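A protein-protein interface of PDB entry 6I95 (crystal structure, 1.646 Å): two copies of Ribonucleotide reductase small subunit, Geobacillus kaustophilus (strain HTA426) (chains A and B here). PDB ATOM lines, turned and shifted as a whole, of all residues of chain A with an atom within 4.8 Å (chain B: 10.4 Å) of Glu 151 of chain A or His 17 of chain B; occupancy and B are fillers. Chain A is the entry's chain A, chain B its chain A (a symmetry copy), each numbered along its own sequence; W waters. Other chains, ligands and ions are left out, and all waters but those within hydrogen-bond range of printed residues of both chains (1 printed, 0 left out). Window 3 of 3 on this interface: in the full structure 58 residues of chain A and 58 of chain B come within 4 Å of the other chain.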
ATOM      1  N   LYS A 146       6.897  28.812 -21.885  1.00  0.00           N
ATOM      2  CA  LYS A 146       5.631  29.487 -22.157  1.00  0.00           C
ATOM      3  C   LYS A 146       4.922  28.884 -23.357  1.00  0.00           C
ATOM      4  O   LYS A 146       3.689  28.742 -23.351  1.00  0.00           O
ATOM      5  CB  LYS A 146       5.879  30.989 -22.360  1.00  0.00           C
ATOM      6  CG  LYS A 146       6.273  31.671 -21.084  1.00  0.00           C
ATOM      7  CD  LYS A 146       6.474  33.160 -21.256  1.00  0.00           C
ATOM      8  CE  LYS A 146       6.760  33.812 -19.936  1.00  0.00           C
ATOM      9  NZ  LYS A 146       7.206  35.222 -20.132  1.00  0.00           N
ATOM     10  N   ARG A 147       5.666  28.512 -24.400  1.00  0.00           N
ATOM     11  CA  ARG A 147       5.010  27.926 -25.558  1.00  0.00           C
ATOM     12  C   ARG A 147       4.256  26.664 -25.175  1.00  0.00           C
ATOM     13  O   ARG A 147       3.191  26.398 -25.730  1.00  0.00           O
ATOM     14  CB  ARG A 147       6.005  27.623 -26.681  1.00  0.00           C
ATOM     15  CG  ARG A 147       5.360  26.970 -27.903  1.00  0.00           C
ATOM     16  CD  ARG A 147       4.241  27.855 -28.545  1.00  0.00           C
ATOM     17  NE  ARG A 147       3.096  27.074 -29.026  1.00  0.00           N
ATOM     18  CZ  ARG A 147       1.925  27.594 -29.408  1.00  0.00           C
ATOM     19  NH1 ARG A 147       1.717  28.909 -29.362  1.00  0.00           N
ATOM     20  NH2 ARG A 147       0.949  26.794 -29.834  1.00  0.00           N
ATOM     21  N   ILE A 148       4.774  25.890 -24.214  1.00  0.00           N
ATOM     22  CA  ILE A 148       4.098  24.668 -23.799  1.00  0.00           C
ATOM     23  C   ILE A 148       2.971  24.981 -22.815  1.00  0.00           C
ATOM     24  O   ILE A 148       1.802  24.641 -23.049  1.00  0.00           O
ATOM     25  CB  ILE A 148       5.101  23.671 -23.192  1.00  0.00           C
ATOM     26  CG1 ILE A 148       6.115  23.246 -24.256  1.00  0.00           C
ATOM     27  CG2 ILE A 148       4.363  22.444 -22.647  1.00  0.00           C
ATOM     28  CD1 ILE A 148       7.324  22.507 -23.683  1.00  0.00           C
ATOM     29  N   PHE A 149       3.298  25.669 -21.721  1.00  0.00           N
ATOM     30  CA  PHE A 149       2.378  25.749 -20.590  1.00  0.00           C
ATOM     31  C   PHE A 149       1.448  26.939 -20.654  1.00  0.00           C
ATOM     32  O   PHE A 149       0.299  26.843 -20.193  1.00  0.00           O
ATOM     33  CB  PHE A 149       3.172  25.779 -19.285  1.00  0.00           C
ATOM     34  CG  PHE A 149       3.802  24.471 -18.972  1.00  0.00           C
ATOM     35  CD1 PHE A 149       3.075  23.494 -18.345  1.00  0.00           C
ATOM     36  CD2 PHE A 149       5.105  24.207 -19.358  1.00  0.00           C
ATOM     37  CE1 PHE A 149       3.623  22.292 -18.106  1.00  0.00           C
ATOM     38  CE2 PHE A 149       5.681  22.978 -19.105  1.00  0.00           C
ATOM     39  CZ  PHE A 149       4.928  22.022 -18.469  1.00  0.00           C
ATOM     40  N   TYR A 150       1.878  28.045 -21.236  1.00  0.00           N
ATOM     41  CA  TYR A 150       0.968  29.167 -21.336  1.00  0.00           C
ATOM     42  C   TYR A 150       0.086  29.084 -22.568  1.00  0.00           C
ATOM     43  O   TYR A 150      -0.983  29.702 -22.563  1.00  0.00           O
ATOM     44  CB  TYR A 150       1.720  30.493 -21.363  1.00  0.00           C
ATOM     45  CG  TYR A 150       2.458  30.905 -20.093  1.00  0.00           C
ATOM     46  CD1 TYR A 150       2.356  32.202 -19.641  1.00  0.00           C
ATOM     47  CD2 TYR A 150       3.291  30.023 -19.386  1.00  0.00           C
ATOM     48  CE1 TYR A 150       3.031  32.634 -18.531  1.00  0.00           C
ATOM     49  CE2 TYR A 150       3.979  30.446 -18.242  1.00  0.00           C
ATOM     50  CZ  TYR A 150       3.843  31.775 -17.830  1.00  0.00           C
ATOM     51  OH  TYR A 150       4.486  32.305 -16.728  1.00  0.00           O
ATOM     52  N   GLU A 151       0.502  28.325 -23.597  1.00  0.00           N
ATOM     53  CA  GLU A 151      -0.137  28.346 -24.919  1.00  0.00           C
ATOM     54  C   GLU A 151      -0.565  26.960 -25.397  1.00  0.00           C
ATOM     55  O   GLU A 151      -1.772  26.702 -25.478  1.00  0.00           O
ATOM     56  CB  GLU A 151       0.807  29.009 -25.928  1.00  0.00           C
ATOM     57  CG  GLU A 151       1.168  30.436 -25.564  1.00  0.00           C
ATOM     58  CD  GLU A 151       2.103  31.075 -26.587  1.00  0.00           C
ATOM     59  OE1 GLU A 151       2.087  30.649 -27.762  1.00  0.00           O
ATOM     60  OE2 GLU A 151       2.873  31.981 -26.214  1.00  0.00           O
ATOM     61  N   ALA A 152       0.369  26.054 -25.731  1.00  0.00           N
ATOM     62  CA  ALA A 152      -0.006  24.822 -26.432  1.00  0.00           C
ATOM     63  C   ALA A 152      -0.926  23.945 -25.588  1.00  0.00           C
ATOM     64  O   ALA A 152      -1.869  23.337 -26.113  1.00  0.00           O
ATOM     65  CB  ALA A 152       1.234  24.016 -26.826  1.00  0.00           C
ATOM     66  N   LEU A 153      -0.617  23.806 -24.284  1.00  0.00           N
ATOM     67  CA  LEU A 153      -1.456  22.972 -23.430  1.00  0.00           C
ATOM     68  C   LEU A 153      -2.878  23.512 -23.358  1.00  0.00           C
ATOM     69  O   LEU A 153      -3.813  22.785 -23.731  1.00  0.00           O
ATOM     70  CB  LEU A 153      -0.798  22.827 -22.055  1.00  0.00           C
ATOM     71  CG  LEU A 153      -1.632  22.108 -21.022  1.00  0.00           C
ATOM     72  CD1 LEU A 153      -1.894  20.631 -21.340  1.00  0.00           C
ATOM     73  CD2 LEU A 153      -0.918  22.240 -19.748  1.00  0.00           C
ATOM     74  N   PRO A 154      -3.119  24.745 -22.914  1.00  0.00           N
ATOM     75  CA  PRO A 154      -4.520  25.202 -22.878  1.00  0.00           C
ATOM     76  C   PRO A 154      -5.194  25.218 -24.241  1.00  0.00           C
ATOM     77  O   PRO A 154      -6.404  24.960 -24.332  1.00  0.00           O
ATOM     78  CB  PRO A 154      -4.410  26.600 -22.253  1.00  0.00           C
ATOM     79  CG  PRO A 154      -2.977  27.037 -22.456  1.00  0.00           C
ATOM     80  CD  PRO A 154      -2.218  25.730 -22.280  1.00  0.00           C
ATOM     81  N   GLU A 155      -4.451  25.459 -25.311  1.00  0.00           N
ATOM     82  CA  GLU A 155      -5.092  25.497 -26.625  1.00  0.00           C
ATOM     83  C   GLU A 155      -5.584  24.118 -27.026  1.00  0.00           C
ATOM     84  O   GLU A 155      -6.717  23.958 -27.516  1.00  0.00           O
ATOM     85  CB  GLU A 155      -4.112  26.035 -27.678  1.00  0.00           C
ATOM     86  CG  GLU A 155      -3.916  27.505 -27.717  1.00  0.00           C
ATOM     87  CD  GLU A 155      -2.865  27.889 -28.761  1.00  0.00           C
ATOM     88  OE1 GLU A 155      -2.424  27.023 -29.555  1.00  0.00           O
ATOM     89  OE2 GLU A 155      -2.463  29.055 -28.767  1.00  0.00           O
ATOM     90  N   VAL B  16      -7.727  29.293 -24.718  1.00  0.00           N
ATOM     91  CA  VAL B  16      -7.010  30.563 -24.633  1.00  0.00           C
ATOM     92  C   VAL B  16      -5.968  30.493 -23.507  1.00  0.00           C
ATOM     93  O   VAL B  16      -6.077  29.713 -22.557  1.00  0.00           O
ATOM     94  CB  VAL B  16      -7.998  31.766 -24.451  1.00  0.00           C
ATOM     95  CG1 VAL B  16      -8.442  31.931 -23.004  1.00  0.00           C
ATOM     96  CG2 VAL B  16      -7.403  33.067 -24.984  1.00  0.00           C
ATOM     97  N   HIS B  17      -4.973  31.358 -23.630  1.00  0.00           N
ATOM     98  CA  HIS B  17      -3.706  31.229 -22.930  1.00  0.00           C
ATOM     99  C   HIS B  17      -3.853  31.408 -21.418  1.00  0.00           C
ATOM    100  O   HIS B  17      -4.846  31.933 -20.906  1.00  0.00           O
ATOM    101  CB  HIS B  17      -2.725  32.262 -23.472  1.00  0.00           C
ATOM    102  CG  HIS B  17      -2.420  32.088 -24.927  1.00  0.00           C
ATOM    103  ND1 HIS B  17      -2.980  31.079 -25.682  1.00  0.00           N
ATOM    104  CD2 HIS B  17      -1.616  32.787 -25.766  1.00  0.00           C
ATOM    105  CE1 HIS B  17      -2.537  31.166 -26.924  1.00  0.00           C
ATOM    106  NE2 HIS B  17      -1.706  32.192 -27.002  1.00  0.00           N
ATOM    107  N   HIS B  18      -2.845  30.943 -20.695  1.00  0.00           N
ATOM    108  CA  HIS B  18      -2.682  31.340 -19.305  1.00  0.00           C
ATOM    109  C   HIS B  18      -1.839  32.612 -19.278  1.00  0.00           C
ATOM    110  O   HIS B  18      -0.784  32.664 -19.909  1.00  0.00           O
ATOM    111  CB  HIS B  18      -1.998  30.250 -18.468  1.00  0.00           C
ATOM    112  CG  HIS B  18      -2.768  28.966 -18.394  1.00  0.00           C
ATOM    113  ND1 HIS B  18      -4.019  28.881 -17.812  1.00  0.00           N
ATOM    114  CD2 HIS B  18      -2.465  27.714 -18.822  1.00  0.00           C
ATOM    115  CE1 HIS B  18      -4.457  27.636 -17.899  1.00  0.00           C
ATOM    116  NE2 HIS B  18      -3.542  26.911 -18.523  1.00  0.00           N
ATOM    117  N   ASP B  19      -2.321  33.630 -18.568  1.00  0.00           N
ATOM    118  CA  ASP B  19      -1.578  34.883 -18.424  1.00  0.00           C
ATOM    119  C   ASP B  19      -0.363  34.700 -17.527  1.00  0.00           C
ATOM    120  O   ASP B  19       0.749  35.114 -17.871  1.00  0.00           O
ATOM    121  CB  ASP B  19      -2.499  35.967 -17.860  1.00  0.00           C
ATOM    122  CG  ASP B  19      -1.743  37.197 -17.419  1.00  0.00           C
ATOM    123  OD1 ASP B  19      -0.748  37.545 -18.087  1.00  0.00           O
ATOM    124  OD2 ASP B  19      -2.138  37.813 -16.402  1.00  0.00           O
ATOM    125  N   GLY B  20      -0.571  34.132 -16.361  1.00  0.00           N
ATOM    126  CA  GLY B  20       0.497  33.571 -15.563  1.00  0.00           C
ATOM    127  C   GLY B  20      -0.156  32.591 -14.640  1.00  0.00           C
ATOM    128  O   GLY B  20      -1.283  32.163 -14.884  1.00  0.00           O
ATOM    129  N   PHE B  21       0.527  32.271 -13.536  1.00  0.00           N
ATOM    130  CA  PHE B  21       0.023  31.316 -12.561  1.00  0.00           C
ATOM    131  C   PHE B  21       0.105  31.899 -11.160  1.00  0.00           C
ATOM    132  O   PHE B  21       1.154  32.413 -10.757  1.00  0.00           O
ATOM    133  CB  PHE B  21       0.824  30.020 -12.694  1.00  0.00           C
ATOM    134  CG  PHE B  21       0.638  29.377 -14.017  1.00  0.00           C
ATOM    135  CD1 PHE B  21      -0.495  28.667 -14.260  1.00  0.00           C
ATOM    136  CD2 PHE B  21       1.544  29.557 -15.048  1.00  0.00           C
ATOM    137  CE1 PHE B  21      -0.713  28.063 -15.491  1.00  0.00           C
ATOM    138  CE2 PHE B  21       1.329  28.947 -16.298  1.00  0.00           C
ATOM    139  CZ  PHE B  21       0.208  28.222 -16.515  1.00  0.00           C
ATOM    140  N   HIS B  95     -15.300  25.195 -14.834  1.00  0.00           N
ATOM    141  CA  HIS B  95     -14.637  25.878 -15.925  1.00  0.00           C
ATOM    142  C   HIS B  95     -14.787  27.384 -15.800  1.00  0.00           C
ATOM    143  O   HIS B  95     -13.812  28.132 -15.948  1.00  0.00           O
ATOM    144  CB  HIS B  95     -15.237  25.419 -17.239  1.00  0.00           C
ATOM    145  CG  HIS B  95     -14.976  26.354 -18.379  1.00  0.00           C
ATOM    146  ND1 HIS B  95     -13.814  26.315 -19.098  1.00  0.00           N
ATOM    147  CD2 HIS B  95     -15.709  27.373 -18.889  1.00  0.00           C
ATOM    148  CE1 HIS B  95     -13.839  27.256 -20.022  1.00  0.00           C
ATOM    149  NE2 HIS B  95     -14.979  27.915 -19.915  1.00  0.00           N
ATOM    150  N   ALA B  98     -12.629  28.738 -13.018  1.00  0.00           N
ATOM    151  CA  ALA B  98     -11.221  28.673 -13.388  1.00  0.00           C
ATOM    152  C   ALA B  98     -10.870  29.804 -14.335  1.00  0.00           C
ATOM    153  O   ALA B  98      -9.839  30.457 -14.175  1.00  0.00           O
ATOM    154  CB  ALA B  98     -10.906  27.321 -14.040  1.00  0.00           C
ATOM    155  N   ARG B  99     -11.743  30.061 -15.308  1.00  0.00           N
ATOM    156  CA  ARG B  99     -11.464  31.092 -16.298  1.00  0.00           C
ATOM    157  C   ARG B  99     -11.443  32.466 -15.658  1.00  0.00           C
ATOM    158  O   ARG B  99     -10.747  33.369 -16.146  1.00  0.00           O
ATOM    159  CB  ARG B  99     -12.503  30.996 -17.422  1.00  0.00           C
ATOM    160  CG  ARG B  99     -12.356  31.948 -18.580  1.00  0.00           C
ATOM    161  CD  ARG B  99     -13.347  31.562 -19.700  1.00  0.00           C
ATOM    162  NE  ARG B  99     -14.717  31.425 -19.196  1.00  0.00           N
ATOM    163  CZ  ARG B  99     -15.727  30.847 -19.851  1.00  0.00           C
ATOM    164  NH1 ARG B  99     -15.550  30.333 -21.066  1.00  0.00           N
ATOM    165  NH2 ARG B  99     -16.929  30.778 -19.282  1.00  0.00           N
ATOM    166  N   GLN B 100     -12.211  32.657 -14.592  1.00  0.00           N
ATOM    167  CA  GLN B 100     -12.179  33.885 -13.805  1.00  0.00           C
ATOM    168  C   GLN B 100     -11.016  33.944 -12.828  1.00  0.00           C
ATOM    169  O   GLN B 100     -10.929  34.902 -12.059  1.00  0.00           O
ATOM    170  CB  GLN B 100     -13.484  34.028 -13.025  1.00  0.00           C
ATOM    171  CG  GLN B 100     -14.723  34.215 -13.913  1.00  0.00           C
ATOM    172  CD  GLN B 100     -15.998  34.367 -13.154  1.00  0.00           C
ATOM    173  OE1 GLN B 100     -16.012  34.381 -11.934  1.00  0.00           O
ATOM    174  NE2 GLN B 100     -17.107  34.502 -13.887  1.00  0.00           N
ATOM    175  N   GLY B 101     -10.151  32.935 -12.811  1.00  0.00           N
ATOM    176  CA  GLY B 101      -8.990  32.947 -11.934  1.00  0.00           C
ATOM    177  C   GLY B 101      -9.256  32.613 -10.484  1.00  0.00           C
ATOM    178  O   GLY B 101      -8.416  32.906  -9.623  1.00  0.00           O
HETATM  179  O   HOH W   1       3.412  32.863 -13.933  1.00  0.00           O
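O of Tyr 150 of chain A lies within hydrogen-bond range of N of His 18 of chain B (2.9 Å).
O of Lys 146 of chain A is in hydrogen-bond range of N of Glu 151 of chain A, at 3.2 Å. OE1 of Glu 155 of chain A is in salt-bridge range of NH2 of Arg 147 of chain A, at 3.4 Å. NE of Arg 147 of chain A lies within salt-bridge range of OE1 of Glu 151 of chain A.
Among the printed residues, merely in contact across the chains: Phe 149 of chain A with His 18 of chain B (3.2 Å), Phe 149 of chain A with Phe 21 of chain B (3.9 Å), Tyr 150 of chain A with His 17 of chain B (3.1 Å), Tyr 150 of chain A with Asp 19 of chain B (3.4 Å), Tyr 150 of chain A with Phe 21 of chain B (3.6 Å), Glu 151 of chain A with His 17 of chain B (3.6 Å), Pro 154 of chain A with Val 16 of chain B (3.5 Å), Pro 154 of chain A with His 18 of chain B (3.7 Å) and Glu 155 of chain A with His 17 of chain B (2.8 Å).
Glu 151 of chain A touches just one residue of chain B: His 17. His 17 of chain B touches just these residues of chain A: Tyr 150 (3.1 Å), Glu 151 (3.6 Å) and Glu 155 (2.8 Å). Ala 152 of chain A touches none of the printed residues of chain B. Printed residues of chain B within 4 Å of Pro 154 of chain A: Val 16 (3.5 Å) and His 18 (3.7 Å). Glu 155 of chain A touches just one residue of chain B: His 17. Of the printed residues of chain B, Phe 149 of chain A touches His 18 (3.2 Å) and Phe 21 (3.9 Å). Printed residues of chain B within 4 Å of Tyr 150 of chain A: His 17 (3.1 Å), His 18 (2.9 Å), Asp 19 (3.4 Å) and Phe 21 (3.6 Å). Printed residues of chain A within 4 Å of Asp 19 of chain B: Tyr 150. His 95 of chain B touches none of the printed residues of chain A. Lys 146 of chain A touches none of the printed residues of chain B. The nearest residue of chain A that does not touch His 17 of chain B is Pro 154 of chain A (4.3 Å). The nearest printed residue of chain B that does not touch Phe 149 of chain A is His 17 of chain B (6.3 Å).
Of the 10 printed residues of chain A, 5 touch a printed residue of chain B. Of the 11 printed residues of chain B, 5 touch a printed residue of chain A. Hydrophobic or aromatic side chains of chain B within 4 Å of the printed part of chain A: His 17, His 18 and Phe 21.
No position is printed for both chains.
Water W1 bridges N of Phe 21 of chain B (3.0 Å) and OH of Tyr 150 of chain A (3.0 Å).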
